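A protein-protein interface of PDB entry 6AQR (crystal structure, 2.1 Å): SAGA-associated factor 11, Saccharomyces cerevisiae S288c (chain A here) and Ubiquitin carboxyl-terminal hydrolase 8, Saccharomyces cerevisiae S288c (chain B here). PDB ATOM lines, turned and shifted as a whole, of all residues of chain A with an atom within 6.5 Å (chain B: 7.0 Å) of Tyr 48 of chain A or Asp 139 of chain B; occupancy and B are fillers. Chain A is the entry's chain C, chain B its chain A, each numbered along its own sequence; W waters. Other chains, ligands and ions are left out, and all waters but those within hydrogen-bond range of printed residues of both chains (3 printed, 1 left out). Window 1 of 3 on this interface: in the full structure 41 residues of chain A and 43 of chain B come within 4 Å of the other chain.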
ATOM      1  N   LEU A  38      22.029  13.459   5.617  1.00  0.00           N
ATOM      2  CA  LEU A  38      20.677  13.926   5.992  1.00  0.00           C
ATOM      3  C   LEU A  38      19.610  13.402   4.964  1.00  0.00           C
ATOM      4  O   LEU A  38      18.501  12.979   5.367  1.00  0.00           O
ATOM      5  CB  LEU A  38      20.586  15.439   6.047  1.00  0.00           C
ATOM      6  CG  LEU A  38      21.313  16.150   7.224  1.00  0.00           C
ATOM      7  CD1 LEU A  38      20.949  17.632   7.245  1.00  0.00           C
ATOM      8  CD2 LEU A  38      21.077  15.465   8.571  1.00  0.00           C
ATOM      9  N   ARG A  46      12.957  18.273   4.522  1.00  0.00           N
ATOM     10  CA  ARG A  46      12.711  19.632   3.968  1.00  0.00           C
ATOM     11  C   ARG A  46      13.568  20.619   4.759  1.00  0.00           C
ATOM     12  O   ARG A  46      13.770  20.446   5.973  1.00  0.00           O
ATOM     13  CB  ARG A  46      11.216  20.040   4.034  1.00  0.00           C
ATOM     14  CG  ARG A  46      10.589  19.824   5.416  1.00  0.00           C
ATOM     15  CD  ARG A  46       9.307  20.619   5.710  1.00  0.00           C
ATOM     16  NE  ARG A  46       9.042  20.677   7.164  1.00  0.00           N
ATOM     17  CZ  ARG A  46       8.694  19.634   7.931  1.00  0.00           C
ATOM     18  NH1 ARG A  46       8.506  19.818   9.232  1.00  0.00           N
ATOM     19  NH2 ARG A  46       8.536  18.403   7.418  1.00  0.00           N
ATOM     20  N   SER A  47      14.096  21.627   4.079  1.00  0.00           N
ATOM     21  CA  SER A  47      14.882  22.649   4.766  1.00  0.00           C
ATOM     22  C   SER A  47      14.010  23.554   5.696  1.00  0.00           C
ATOM     23  O   SER A  47      12.783  23.579   5.589  1.00  0.00           O
ATOM     24  CB  SER A  47      15.742  23.441   3.783  1.00  0.00           C
ATOM     25  OG  SER A  47      14.924  24.121   2.875  1.00  0.00           O
ATOM     26  N   TYR A  48      14.658  24.191   6.667  1.00  0.00           N
ATOM     27  CA  TYR A  48      14.010  25.086   7.617  1.00  0.00           C
ATOM     28  C   TYR A  48      13.419  26.212   6.818  1.00  0.00           C
ATOM     29  O   TYR A  48      14.070  26.784   5.937  1.00  0.00           O
ATOM     30  CB  TYR A  48      15.031  25.611   8.664  1.00  0.00           C
ATOM     31  CG  TYR A  48      15.559  24.517   9.576  1.00  0.00           C
ATOM     32  CD1 TYR A  48      14.664  23.732  10.360  1.00  0.00           C
ATOM     33  CD2 TYR A  48      16.921  24.217   9.618  1.00  0.00           C
ATOM     34  CE1 TYR A  48      15.114  22.697  11.175  1.00  0.00           C
ATOM     35  CE2 TYR A  48      17.399  23.190  10.435  1.00  0.00           C
ATOM     36  CZ  TYR A  48      16.488  22.444  11.232  1.00  0.00           C
ATOM     37  OH  TYR A  48      16.971  21.424  12.086  1.00  0.00           O
ATOM     38  N   TYR A  49      12.176  26.532   7.087  1.00  0.00           N
ATOM     39  CA  TYR A  49      11.580  27.602   6.346  1.00  0.00           C
ATOM     40  C   TYR A  49      12.272  28.908   6.611  1.00  0.00           C
ATOM     41  O   TYR A  49      12.424  29.349   7.784  1.00  0.00           O
ATOM     42  CB  TYR A  49      10.138  27.746   6.736  1.00  0.00           C
ATOM     43  CG  TYR A  49       9.370  28.666   5.850  1.00  0.00           C
ATOM     44  CD1 TYR A  49       9.173  29.975   6.222  1.00  0.00           C
ATOM     45  CD2 TYR A  49       8.819  28.228   4.618  1.00  0.00           C
ATOM     46  CE1 TYR A  49       8.450  30.843   5.451  1.00  0.00           C
ATOM     47  CE2 TYR A  49       8.090  29.108   3.816  1.00  0.00           C
ATOM     48  CZ  TYR A  49       7.912  30.416   4.251  1.00  0.00           C
ATOM     49  OH  TYR A  49       7.197  31.361   3.558  1.00  0.00           O
ATOM     50  N   PHE A  50      12.638  29.565   5.519  1.00  0.00           N
ATOM     51  CA  PHE A  50      13.201  30.908   5.580  1.00  0.00           C
ATOM     52  C   PHE A  50      12.133  31.851   5.031  1.00  0.00           C
ATOM     53  O   PHE A  50      11.589  31.599   3.985  1.00  0.00           O
ATOM     54  CB  PHE A  50      14.527  30.942   4.799  1.00  0.00           C
ATOM     55  CG  PHE A  50      15.202  32.278   4.755  1.00  0.00           C
ATOM     56  CD1 PHE A  50      15.914  32.663   3.607  1.00  0.00           C
ATOM     57  CD2 PHE A  50      15.159  33.167   5.848  1.00  0.00           C
ATOM     58  CE1 PHE A  50      16.566  33.905   3.552  1.00  0.00           C
ATOM     59  CE2 PHE A  50      15.800  34.408   5.794  1.00  0.00           C
ATOM     60  CZ  PHE A  50      16.507  34.776   4.648  1.00  0.00           C
ATOM     61  N   ASP A  57       7.882  30.953  11.236  1.00  0.00           N
ATOM     62  CA  ASP A  57       8.917  30.229  11.949  1.00  0.00           C
ATOM     63  C   ASP A  57       9.606  29.186  11.067  1.00  0.00           C
ATOM     64  O   ASP A  57       9.322  29.108   9.844  1.00  0.00           O
ATOM     65  CB  ASP A  57       8.381  29.678  13.271  1.00  0.00           C
ATOM     66  CG  ASP A  57       7.496  28.447  13.108  1.00  0.00           C
ATOM     67  OD1 ASP A  57       7.294  27.967  11.970  1.00  0.00           O
ATOM     68  OD2 ASP A  57       7.027  27.948  14.160  1.00  0.00           O
ATOM     69  N   ILE A  58      10.494  28.375  11.654  1.00  0.00           N
ATOM     70  CA  ILE A  58      11.247  27.416  10.854  1.00  0.00           C
ATOM     71  C   ILE A  58      10.363  26.304  10.244  1.00  0.00           C
ATOM     72  O   ILE A  58      10.812  25.566   9.347  1.00  0.00           O
ATOM     73  CB  ILE A  58      12.418  26.832  11.644  1.00  0.00           C
ATOM     74  CG1 ILE A  58      11.865  26.115  12.879  1.00  0.00           C
ATOM     75  CG2 ILE A  58      13.373  27.990  11.972  1.00  0.00           C
ATOM     76  CD1 ILE A  58      12.845  25.248  13.629  1.00  0.00           C
ATOM     77  N   ASN A  59       9.129  26.204  10.731  1.00  0.00           N
ATOM     78  CA  ASN A  59       8.092  25.312  10.129  1.00  0.00           C
ATOM     79  C   ASN A  59       7.064  25.945   9.118  1.00  0.00           C
ATOM     80  O   ASN A  59       6.155  25.243   8.611  1.00  0.00           O
ATOM     81  CB  ASN A  59       7.351  24.590  11.264  1.00  0.00           C
ATOM     82  CG  ASN A  59       8.255  23.627  11.972  1.00  0.00           C
ATOM     83  OD1 ASN A  59       8.891  22.800  11.336  1.00  0.00           O
ATOM     84  ND2 ASN A  59       8.371  23.760  13.268  1.00  0.00           N
ATOM     85  N   PRO B 133      18.886  10.452  15.564  1.00  0.00           N
ATOM     86  CA  PRO B 133      17.922  11.487  15.967  1.00  0.00           C
ATOM     87  C   PRO B 133      16.735  11.554  15.032  1.00  0.00           C
ATOM     88  O   PRO B 133      16.867  11.212  13.813  1.00  0.00           O
ATOM     89  CB  PRO B 133      18.724  12.806  15.811  1.00  0.00           C
ATOM     90  CG  PRO B 133      20.125  12.426  15.712  1.00  0.00           C
ATOM     91  CD  PRO B 133      20.194  11.005  15.204  1.00  0.00           C
ATOM     92  N   SER B 134      15.603  12.030  15.544  1.00  0.00           N
ATOM     93  CA  SER B 134      14.458  12.286  14.668  1.00  0.00           C
ATOM     94  C   SER B 134      14.687  13.588  13.922  1.00  0.00           C
ATOM     95  O   SER B 134      15.445  14.488  14.384  1.00  0.00           O
ATOM     96  CB  SER B 134      13.121  12.266  15.420  1.00  0.00           C
ATOM     97  OG  SER B 134      12.982  13.478  16.147  1.00  0.00           O
ATOM     98  N   MET B 135      14.052  13.681  12.756  1.00  0.00           N
ATOM     99  CA  MET B 135      14.273  14.753  11.834  1.00  0.00           C
ATOM    100  C   MET B 135      14.119  16.152  12.488  1.00  0.00           C
ATOM    101  O   MET B 135      15.012  17.007  12.360  1.00  0.00           O
ATOM    102  CB  MET B 135      13.338  14.642  10.659  1.00  0.00           C
ATOM    103  CG  MET B 135      13.634  15.692   9.590  1.00  0.00           C
ATOM    104  SD  MET B 135      12.481  15.597   8.169  1.00  0.00           S
ATOM    105  CE  MET B 135      10.991  16.313   8.883  1.00  0.00           C
ATOM    106  N   GLU B 136      13.000  16.380  13.133  1.00  0.00           N
ATOM    107  CA  GLU B 136      12.659  17.740  13.601  1.00  0.00           C
ATOM    108  C   GLU B 136      13.446  18.077  14.921  1.00  0.00           C
ATOM    109  O   GLU B 136      13.498  19.194  15.334  1.00  0.00           O
ATOM    110  CB  GLU B 136      11.132  17.958  13.677  1.00  0.00           C
ATOM    111  CG  GLU B 136      10.312  16.890  14.418  1.00  0.00           C
ATOM    112  CD  GLU B 136       9.697  15.811  13.510  1.00  0.00           C
ATOM    113  OE1 GLU B 136      10.412  15.123  12.738  1.00  0.00           O
ATOM    114  OE2 GLU B 136       8.464  15.622  13.599  1.00  0.00           O
ATOM    115  N   ARG B 137      14.063  17.077  15.536  1.00  0.00           N
ATOM    116  CA  ARG B 137      14.795  17.259  16.801  1.00  0.00           C
ATOM    117  C   ARG B 137      16.304  17.340  16.597  1.00  0.00           C
ATOM    118  O   ARG B 137      17.037  17.693  17.534  1.00  0.00           O
ATOM    119  CB  ARG B 137      14.435  16.198  17.908  1.00  0.00           C
ATOM    120  CG  ARG B 137      12.975  15.878  18.188  1.00  0.00           C
ATOM    121  CD  ARG B 137      12.063  16.974  18.774  1.00  0.00           C
ATOM    122  NE  ARG B 137      12.757  18.211  18.859  1.00  0.00           N
ATOM    123  CZ  ARG B 137      12.429  19.348  18.280  1.00  0.00           C
ATOM    124  NH1 ARG B 137      11.328  19.469  17.552  1.00  0.00           N
ATOM    125  NH2 ARG B 137      13.247  20.377  18.498  1.00  0.00           N
ATOM    126  N   ARG B 138      16.771  17.056  15.377  1.00  0.00           N
ATOM    127  CA  ARG B 138      18.192  16.774  15.167  1.00  0.00           C
ATOM    128  C   ARG B 138      19.073  18.010  15.497  1.00  0.00           C
ATOM    129  O   ARG B 138      20.188  17.792  15.848  1.00  0.00           O
ATOM    130  CB  ARG B 138      18.473  16.380  13.709  1.00  0.00           C
ATOM    131  CG  ARG B 138      18.348  17.527  12.689  1.00  0.00           C
ATOM    132  CD  ARG B 138      18.404  16.990  11.230  1.00  0.00           C
ATOM    133  NE  ARG B 138      18.518  18.113  10.307  1.00  0.00           N
ATOM    134  CZ  ARG B 138      17.484  18.778   9.781  1.00  0.00           C
ATOM    135  NH1 ARG B 138      16.246  18.434  10.015  1.00  0.00           N
ATOM    136  NH2 ARG B 138      17.711  19.774   8.978  1.00  0.00           N
ATOM    137  N   ASP B 139      18.546  19.244  15.358  1.00  0.00           N
ATOM    138  CA  ASP B 139      19.350  20.441  15.664  1.00  0.00           C
ATOM    139  C   ASP B 139      18.935  21.085  17.011  1.00  0.00           C
ATOM    140  O   ASP B 139      19.447  22.141  17.339  1.00  0.00           O
ATOM    141  CB  ASP B 139      19.339  21.462  14.519  1.00  0.00           C
ATOM    142  CG  ASP B 139      20.014  20.908  13.255  1.00  0.00           C
ATOM    143  OD1 ASP B 139      19.329  20.866  12.213  1.00  0.00           O
ATOM    144  OD2 ASP B 139      21.188  20.458  13.315  1.00  0.00           O
ATOM    145  N   GLY B 140      18.038  20.420  17.759  1.00  0.00           N
ATOM    146  CA  GLY B 140      17.504  20.882  19.065  1.00  0.00           C
ATOM    147  C   GLY B 140      16.777  22.215  18.950  1.00  0.00           C
ATOM    148  O   GLY B 140      16.806  23.003  19.874  1.00  0.00           O
ATOM    149  N   LEU B 141      16.172  22.513  17.814  1.00  0.00           N
ATOM    150  CA  LEU B 141      15.551  23.868  17.633  1.00  0.00           C
ATOM    151  C   LEU B 141      14.171  23.803  18.148  1.00  0.00           C
ATOM    152  O   LEU B 141      13.383  22.981  17.693  1.00  0.00           O
ATOM    153  CB  LEU B 141      15.547  24.298  16.158  1.00  0.00           C
ATOM    154  CG  LEU B 141      16.972  24.455  15.625  1.00  0.00           C
ATOM    155  CD1 LEU B 141      17.046  24.561  14.102  1.00  0.00           C
ATOM    156  CD2 LEU B 141      17.574  25.725  16.237  1.00  0.00           C
ATOM    157  N   SER B 142      13.859  24.640  19.114  1.00  0.00           N
ATOM    158  CA  SER B 142      12.508  24.607  19.678  1.00  0.00           C
ATOM    159  C   SER B 142      12.295  25.860  20.504  1.00  0.00           C
ATOM    160  O   SER B 142      13.230  26.380  21.082  1.00  0.00           O
ATOM    161  CB  SER B 142      12.361  23.318  20.525  1.00  0.00           C
ATOM    162  OG  SER B 142      11.092  23.134  21.079  1.00  0.00           O
ATOM    163  N   ILE B 161      22.039  25.965  25.291  1.00  0.00           N
ATOM    164  CA  ILE B 161      21.842  24.641  24.660  1.00  0.00           C
ATOM    165  C   ILE B 161      22.297  24.568  23.193  1.00  0.00           C
ATOM    166  O   ILE B 161      22.271  23.508  22.570  1.00  0.00           O
ATOM    167  CB  ILE B 161      20.435  24.078  24.875  1.00  0.00           C
ATOM    168  CG1 ILE B 161      19.386  24.986  24.251  1.00  0.00           C
ATOM    169  CG2 ILE B 161      20.194  23.888  26.360  1.00  0.00           C
ATOM    170  CD1 ILE B 161      18.958  24.532  22.879  1.00  0.00           C
ATOM    171  N   HIS B 162      22.696  25.689  22.635  1.00  0.00           N
ATOM    172  CA  HIS B 162      23.417  25.696  21.386  1.00  0.00           C
ATOM    173  C   HIS B 162      24.949  25.921  21.543  1.00  0.00           C
ATOM    174  O   HIS B 162      25.640  26.081  20.549  1.00  0.00           O
ATOM    175  CB  HIS B 162      22.767  26.688  20.436  1.00  0.00           C
ATOM    176  CG  HIS B 162      21.402  26.226  20.024  1.00  0.00           C
ATOM    177  ND1 HIS B 162      21.208  25.071  19.284  1.00  0.00           N
ATOM    178  CD2 HIS B 162      20.175  26.737  20.267  1.00  0.00           C
ATOM    179  CE1 HIS B 162      19.908  24.874  19.131  1.00  0.00           C
ATOM    180  NE2 HIS B 162      19.261  25.876  19.707  1.00  0.00           N
ATOM    181  N   LEU B 199      14.721  18.609  23.874  1.00  0.00           N
ATOM    182  CA  LEU B 199      14.865  19.371  22.607  1.00  0.00           C
ATOM    183  C   LEU B 199      15.575  18.509  21.550  1.00  0.00           C
ATOM    184  O   LEU B 199      15.335  18.680  20.398  1.00  0.00           O
ATOM    185  CB  LEU B 199      15.668  20.693  22.809  1.00  0.00           C
ATOM    186  CG  LEU B 199      14.733  21.894  23.083  1.00  0.00           C
ATOM    187  CD1 LEU B 199      13.784  21.623  24.240  1.00  0.00           C
ATOM    188  CD2 LEU B 199      15.538  23.124  23.346  1.00  0.00           C
ATOM    189  N   TYR B 200      16.460  17.612  21.944  1.00  0.00           N
ATOM    190  CA  TYR B 200      17.195  16.792  20.976  1.00  0.00           C
ATOM    191  C   TYR B 200      16.751  15.319  20.978  1.00  0.00           C
ATOM    192  O   TYR B 200      17.052  14.592  20.027  1.00  0.00           O
ATOM    193  CB  TYR B 200      18.702  16.787  21.272  1.00  0.00           C
ATOM    194  CG  TYR B 200      19.461  18.105  21.029  1.00  0.00           C
ATOM    195  CD1 TYR B 200      19.539  19.070  22.020  1.00  0.00           C
ATOM    196  CD2 TYR B 200      20.133  18.352  19.795  1.00  0.00           C
ATOM    197  CE1 TYR B 200      20.237  20.280  21.809  1.00  0.00           C
ATOM    198  CE2 TYR B 200      20.860  19.538  19.589  1.00  0.00           C
ATOM    199  CZ  TYR B 200      20.892  20.498  20.603  1.00  0.00           C
ATOM    200  OH  TYR B 200      21.587  21.650  20.424  1.00  0.00           O
ATOM    201  N   ILE B 439      24.594  27.628  14.217  1.00  0.00           N
ATOM    202  CA  ILE B 439      24.824  26.150  14.269  1.00  0.00           C
ATOM    203  C   ILE B 439      25.633  25.750  13.004  1.00  0.00           C
ATOM    204  O   ILE B 439      26.084  26.657  12.263  1.00  0.00           O
ATOM    205  CB  ILE B 439      23.495  25.367  14.375  1.00  0.00           C
ATOM    206  CG1 ILE B 439      22.640  25.557  13.114  1.00  0.00           C
ATOM    207  CG2 ILE B 439      22.724  25.783  15.636  1.00  0.00           C
ATOM    208  CD1 ILE B 439      21.621  24.453  12.894  1.00  0.00           C
ATOM    209  N   SER B 440      25.919  24.451  12.795  1.00  0.00           N
ATOM    210  CA  SER B 440      26.748  24.057  11.644  1.00  0.00           C
ATOM    211  C   SER B 440      26.107  24.491  10.322  1.00  0.00           C
ATOM    212  O   SER B 440      24.897  24.766  10.274  1.00  0.00           O
ATOM    213  CB  SER B 440      27.001  22.535  11.606  1.00  0.00           C
ATOM    214  OG  SER B 440      25.755  21.884  11.616  1.00  0.00           O
ATOM    215  N   GLN B 443      24.401  28.452   9.456  1.00  0.00           N
ATOM    216  CA  GLN B 443      23.014  28.900   9.574  1.00  0.00           C
ATOM    217  C   GLN B 443      22.796  29.611  10.929  1.00  0.00           C
ATOM    218  O   GLN B 443      23.209  29.096  11.937  1.00  0.00           O
ATOM    219  CB  GLN B 443      22.084  27.666   9.601  1.00  0.00           C
ATOM    220  CG  GLN B 443      22.327  26.469   8.633  1.00  0.00           C
ATOM    221  CD  GLN B 443      21.374  25.265   8.937  1.00  0.00           C
ATOM    222  OE1 GLN B 443      20.143  25.383   8.825  1.00  0.00           O
ATOM    223  NE2 GLN B 443      21.954  24.111   9.352  1.00  0.00           N
ATOM    224  N   PHE B 445      19.828  31.194  13.680  1.00  0.00           N
ATOM    225  CA  PHE B 445      18.426  31.203  14.054  1.00  0.00           C
ATOM    226  C   PHE B 445      18.189  32.260  15.096  1.00  0.00           C
ATOM    227  O   PHE B 445      19.098  32.578  15.880  1.00  0.00           O
ATOM    228  CB  PHE B 445      18.038  29.805  14.567  1.00  0.00           C
ATOM    229  CG  PHE B 445      18.112  28.762  13.474  1.00  0.00           C
ATOM    230  CD1 PHE B 445      16.989  28.531  12.649  1.00  0.00           C
ATOM    231  CD2 PHE B 445      19.299  28.034  13.251  1.00  0.00           C
ATOM    232  CE1 PHE B 445      17.048  27.654  11.580  1.00  0.00           C
ATOM    233  CE2 PHE B 445      19.343  27.094  12.204  1.00  0.00           C
ATOM    234  CZ  PHE B 445      18.223  26.928  11.377  1.00  0.00           C
ATOM    235  N   PHE B 447      15.667  33.402  18.217  1.00  0.00           N
ATOM    236  CA  PHE B 447      14.822  32.768  19.240  1.00  0.00           C
ATOM    237  C   PHE B 447      14.084  33.835  19.983  1.00  0.00           C
ATOM    238  O   PHE B 447      14.674  34.583  20.773  1.00  0.00           O
ATOM    239  CB  PHE B 447      15.639  31.943  20.257  1.00  0.00           C
ATOM    240  CG  PHE B 447      16.403  30.842  19.620  1.00  0.00           C
ATOM    241  CD1 PHE B 447      17.592  31.108  18.939  1.00  0.00           C
ATOM    242  CD2 PHE B 447      15.855  29.538  19.546  1.00  0.00           C
ATOM    243  CE1 PHE B 447      18.304  30.070  18.288  1.00  0.00           C
ATOM    244  CE2 PHE B 447      16.552  28.533  18.877  1.00  0.00           C
ATOM    245  CZ  PHE B 447      17.752  28.770  18.273  1.00  0.00           C
ATOM    246  N   SER B 454      14.456  31.295  11.011  1.00  0.00           N
ATOM    247  CA  SER B 454      15.665  31.296  10.231  1.00  0.00           C
ATOM    248  C   SER B 454      16.025  32.759   9.880  1.00  0.00           C
ATOM    249  O   SER B 454      15.152  33.579   9.654  1.00  0.00           O
ATOM    250  CB  SER B 454      15.411  30.420   8.975  1.00  0.00           C
ATOM    251  OG  SER B 454      16.551  30.501   8.089  1.00  0.00           O
HETATM  252  O   HOH W   1      11.821  31.307   9.589  1.00  0.00           O
HETATM  253  O   HOH W   2      13.558  19.416   9.209  1.00  0.00           O
HETATM  254  O   HOH W   3      15.611  21.243   8.175  1.00  0.00           O
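Hydrophobic or aromatic side chains of chain B that line the printed part of chain A: Met 135, Leu 141 and Phe 445.
Among the printed residues, 12 pairs touch across the chains.
Among the printed residues, no Asp or Glu carboxylate lies within 4 Å of a Lys or Arg side-chain nitrogen of the other chain.
NE of Arg 138 of chain B touches CD1 of Leu 38 of chain A (3.9 Å).
Met 135 of chain B touches Arg 46 of chain A.
CZ of Arg 138 of chain B touches OH of Tyr 48 of chain A (3.5 Å).
Tyr 48 of chain A touches Gln 443 of chain B.
CZ of Phe 445 of chain B touches CD2 of Tyr 48 of chain A, 3.5 Å away.
Tyr 49 of chain A touches Ser 454 of chain B.
CD2 of Phe 50 of chain A touches OG of Ser 454 of chain B, at 3.8 Å.
Leu 141 of chain B touches Ile 58 of chain A.
CG2 of Ile 58 of chain A touches CE1 of Phe 445 of chain B, at 3.7 Å.
Ile 58 of chain A touches Ser 454 of chain B.
Printed residues of chain B within 4 Å of Leu 38 of chain A: Arg 138 (3.9 Å).
Of chain B, only Arg 138, Asp 139, Leu 141, Gln 443 and Phe 445 come within 4 Å of Tyr 48 of chain A.
Of the printed residues of chain B, Ile 58 of chain A touches Leu 141, Phe 445 and Ser 454.
Asp 139 of chain B touches one residue of chain A.
Of the printed residues of chain A, Leu 141 of chain B touches Tyr 48 (3.6 Å) and Ile 58 (3.8 Å).
The nearest residue of chain A that does not touch Asp 139 of chain B is Leu 38 of chain A (6.1 Å).
The nearest printed residue of chain A that does not touch Leu 141 of chain B is Asn 59 of chain A (6.7 Å).
OH of Tyr 48 of chain A sits at hydrogen-bond distance from OD1 of Asp 139 of chain B (2.4 Å).
NH1 of Arg 138 of chain B sits at hydrogen-bond distance from O of Met 135 of chain B.
The guanidinium group of Arg 137 of chain B lies within hydrogen-bond range of the backbone carbonyl oxygen of Leu 141 of chain B (2.7 Å).
The guanidinium group of Arg 138 of chain B is in salt-bridge range of the side-chain carboxylate of Asp 139 of chain B, at 3.4 Å.
O of Ser 440 of chain B lies within hydrogen-bond range of NE2 of Gln 443 of chain B (3.2 Å).
The backbone NH (N) of Tyr 49 of chain A sits at hydrogen-bond distance from the backbone carbonyl oxygen (O) of Ile 58 of chain A (2.8 Å).
Water W3 lies within hydrogen-bond range of the guanidinium group (NH2) of Arg 138 of chain B, the backbone carbonyl oxygen (O) of Arg 46 of chain A and the backbone NH (N) of Tyr 48 of chain A.
Water W1 lies within hydrogen-bond range of the backbone carbonyl oxygen (O) of Tyr 49 of chain A, the backbone NH (N) of Ser 454 of chain B and the backbone carbonyl oxygen (O) of Asp 57 of chain A.
Water W2 bridges NH1 of Arg 138 of chain B (3.0 Å) and O of Arg 46 of chain A (3.4 Å).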
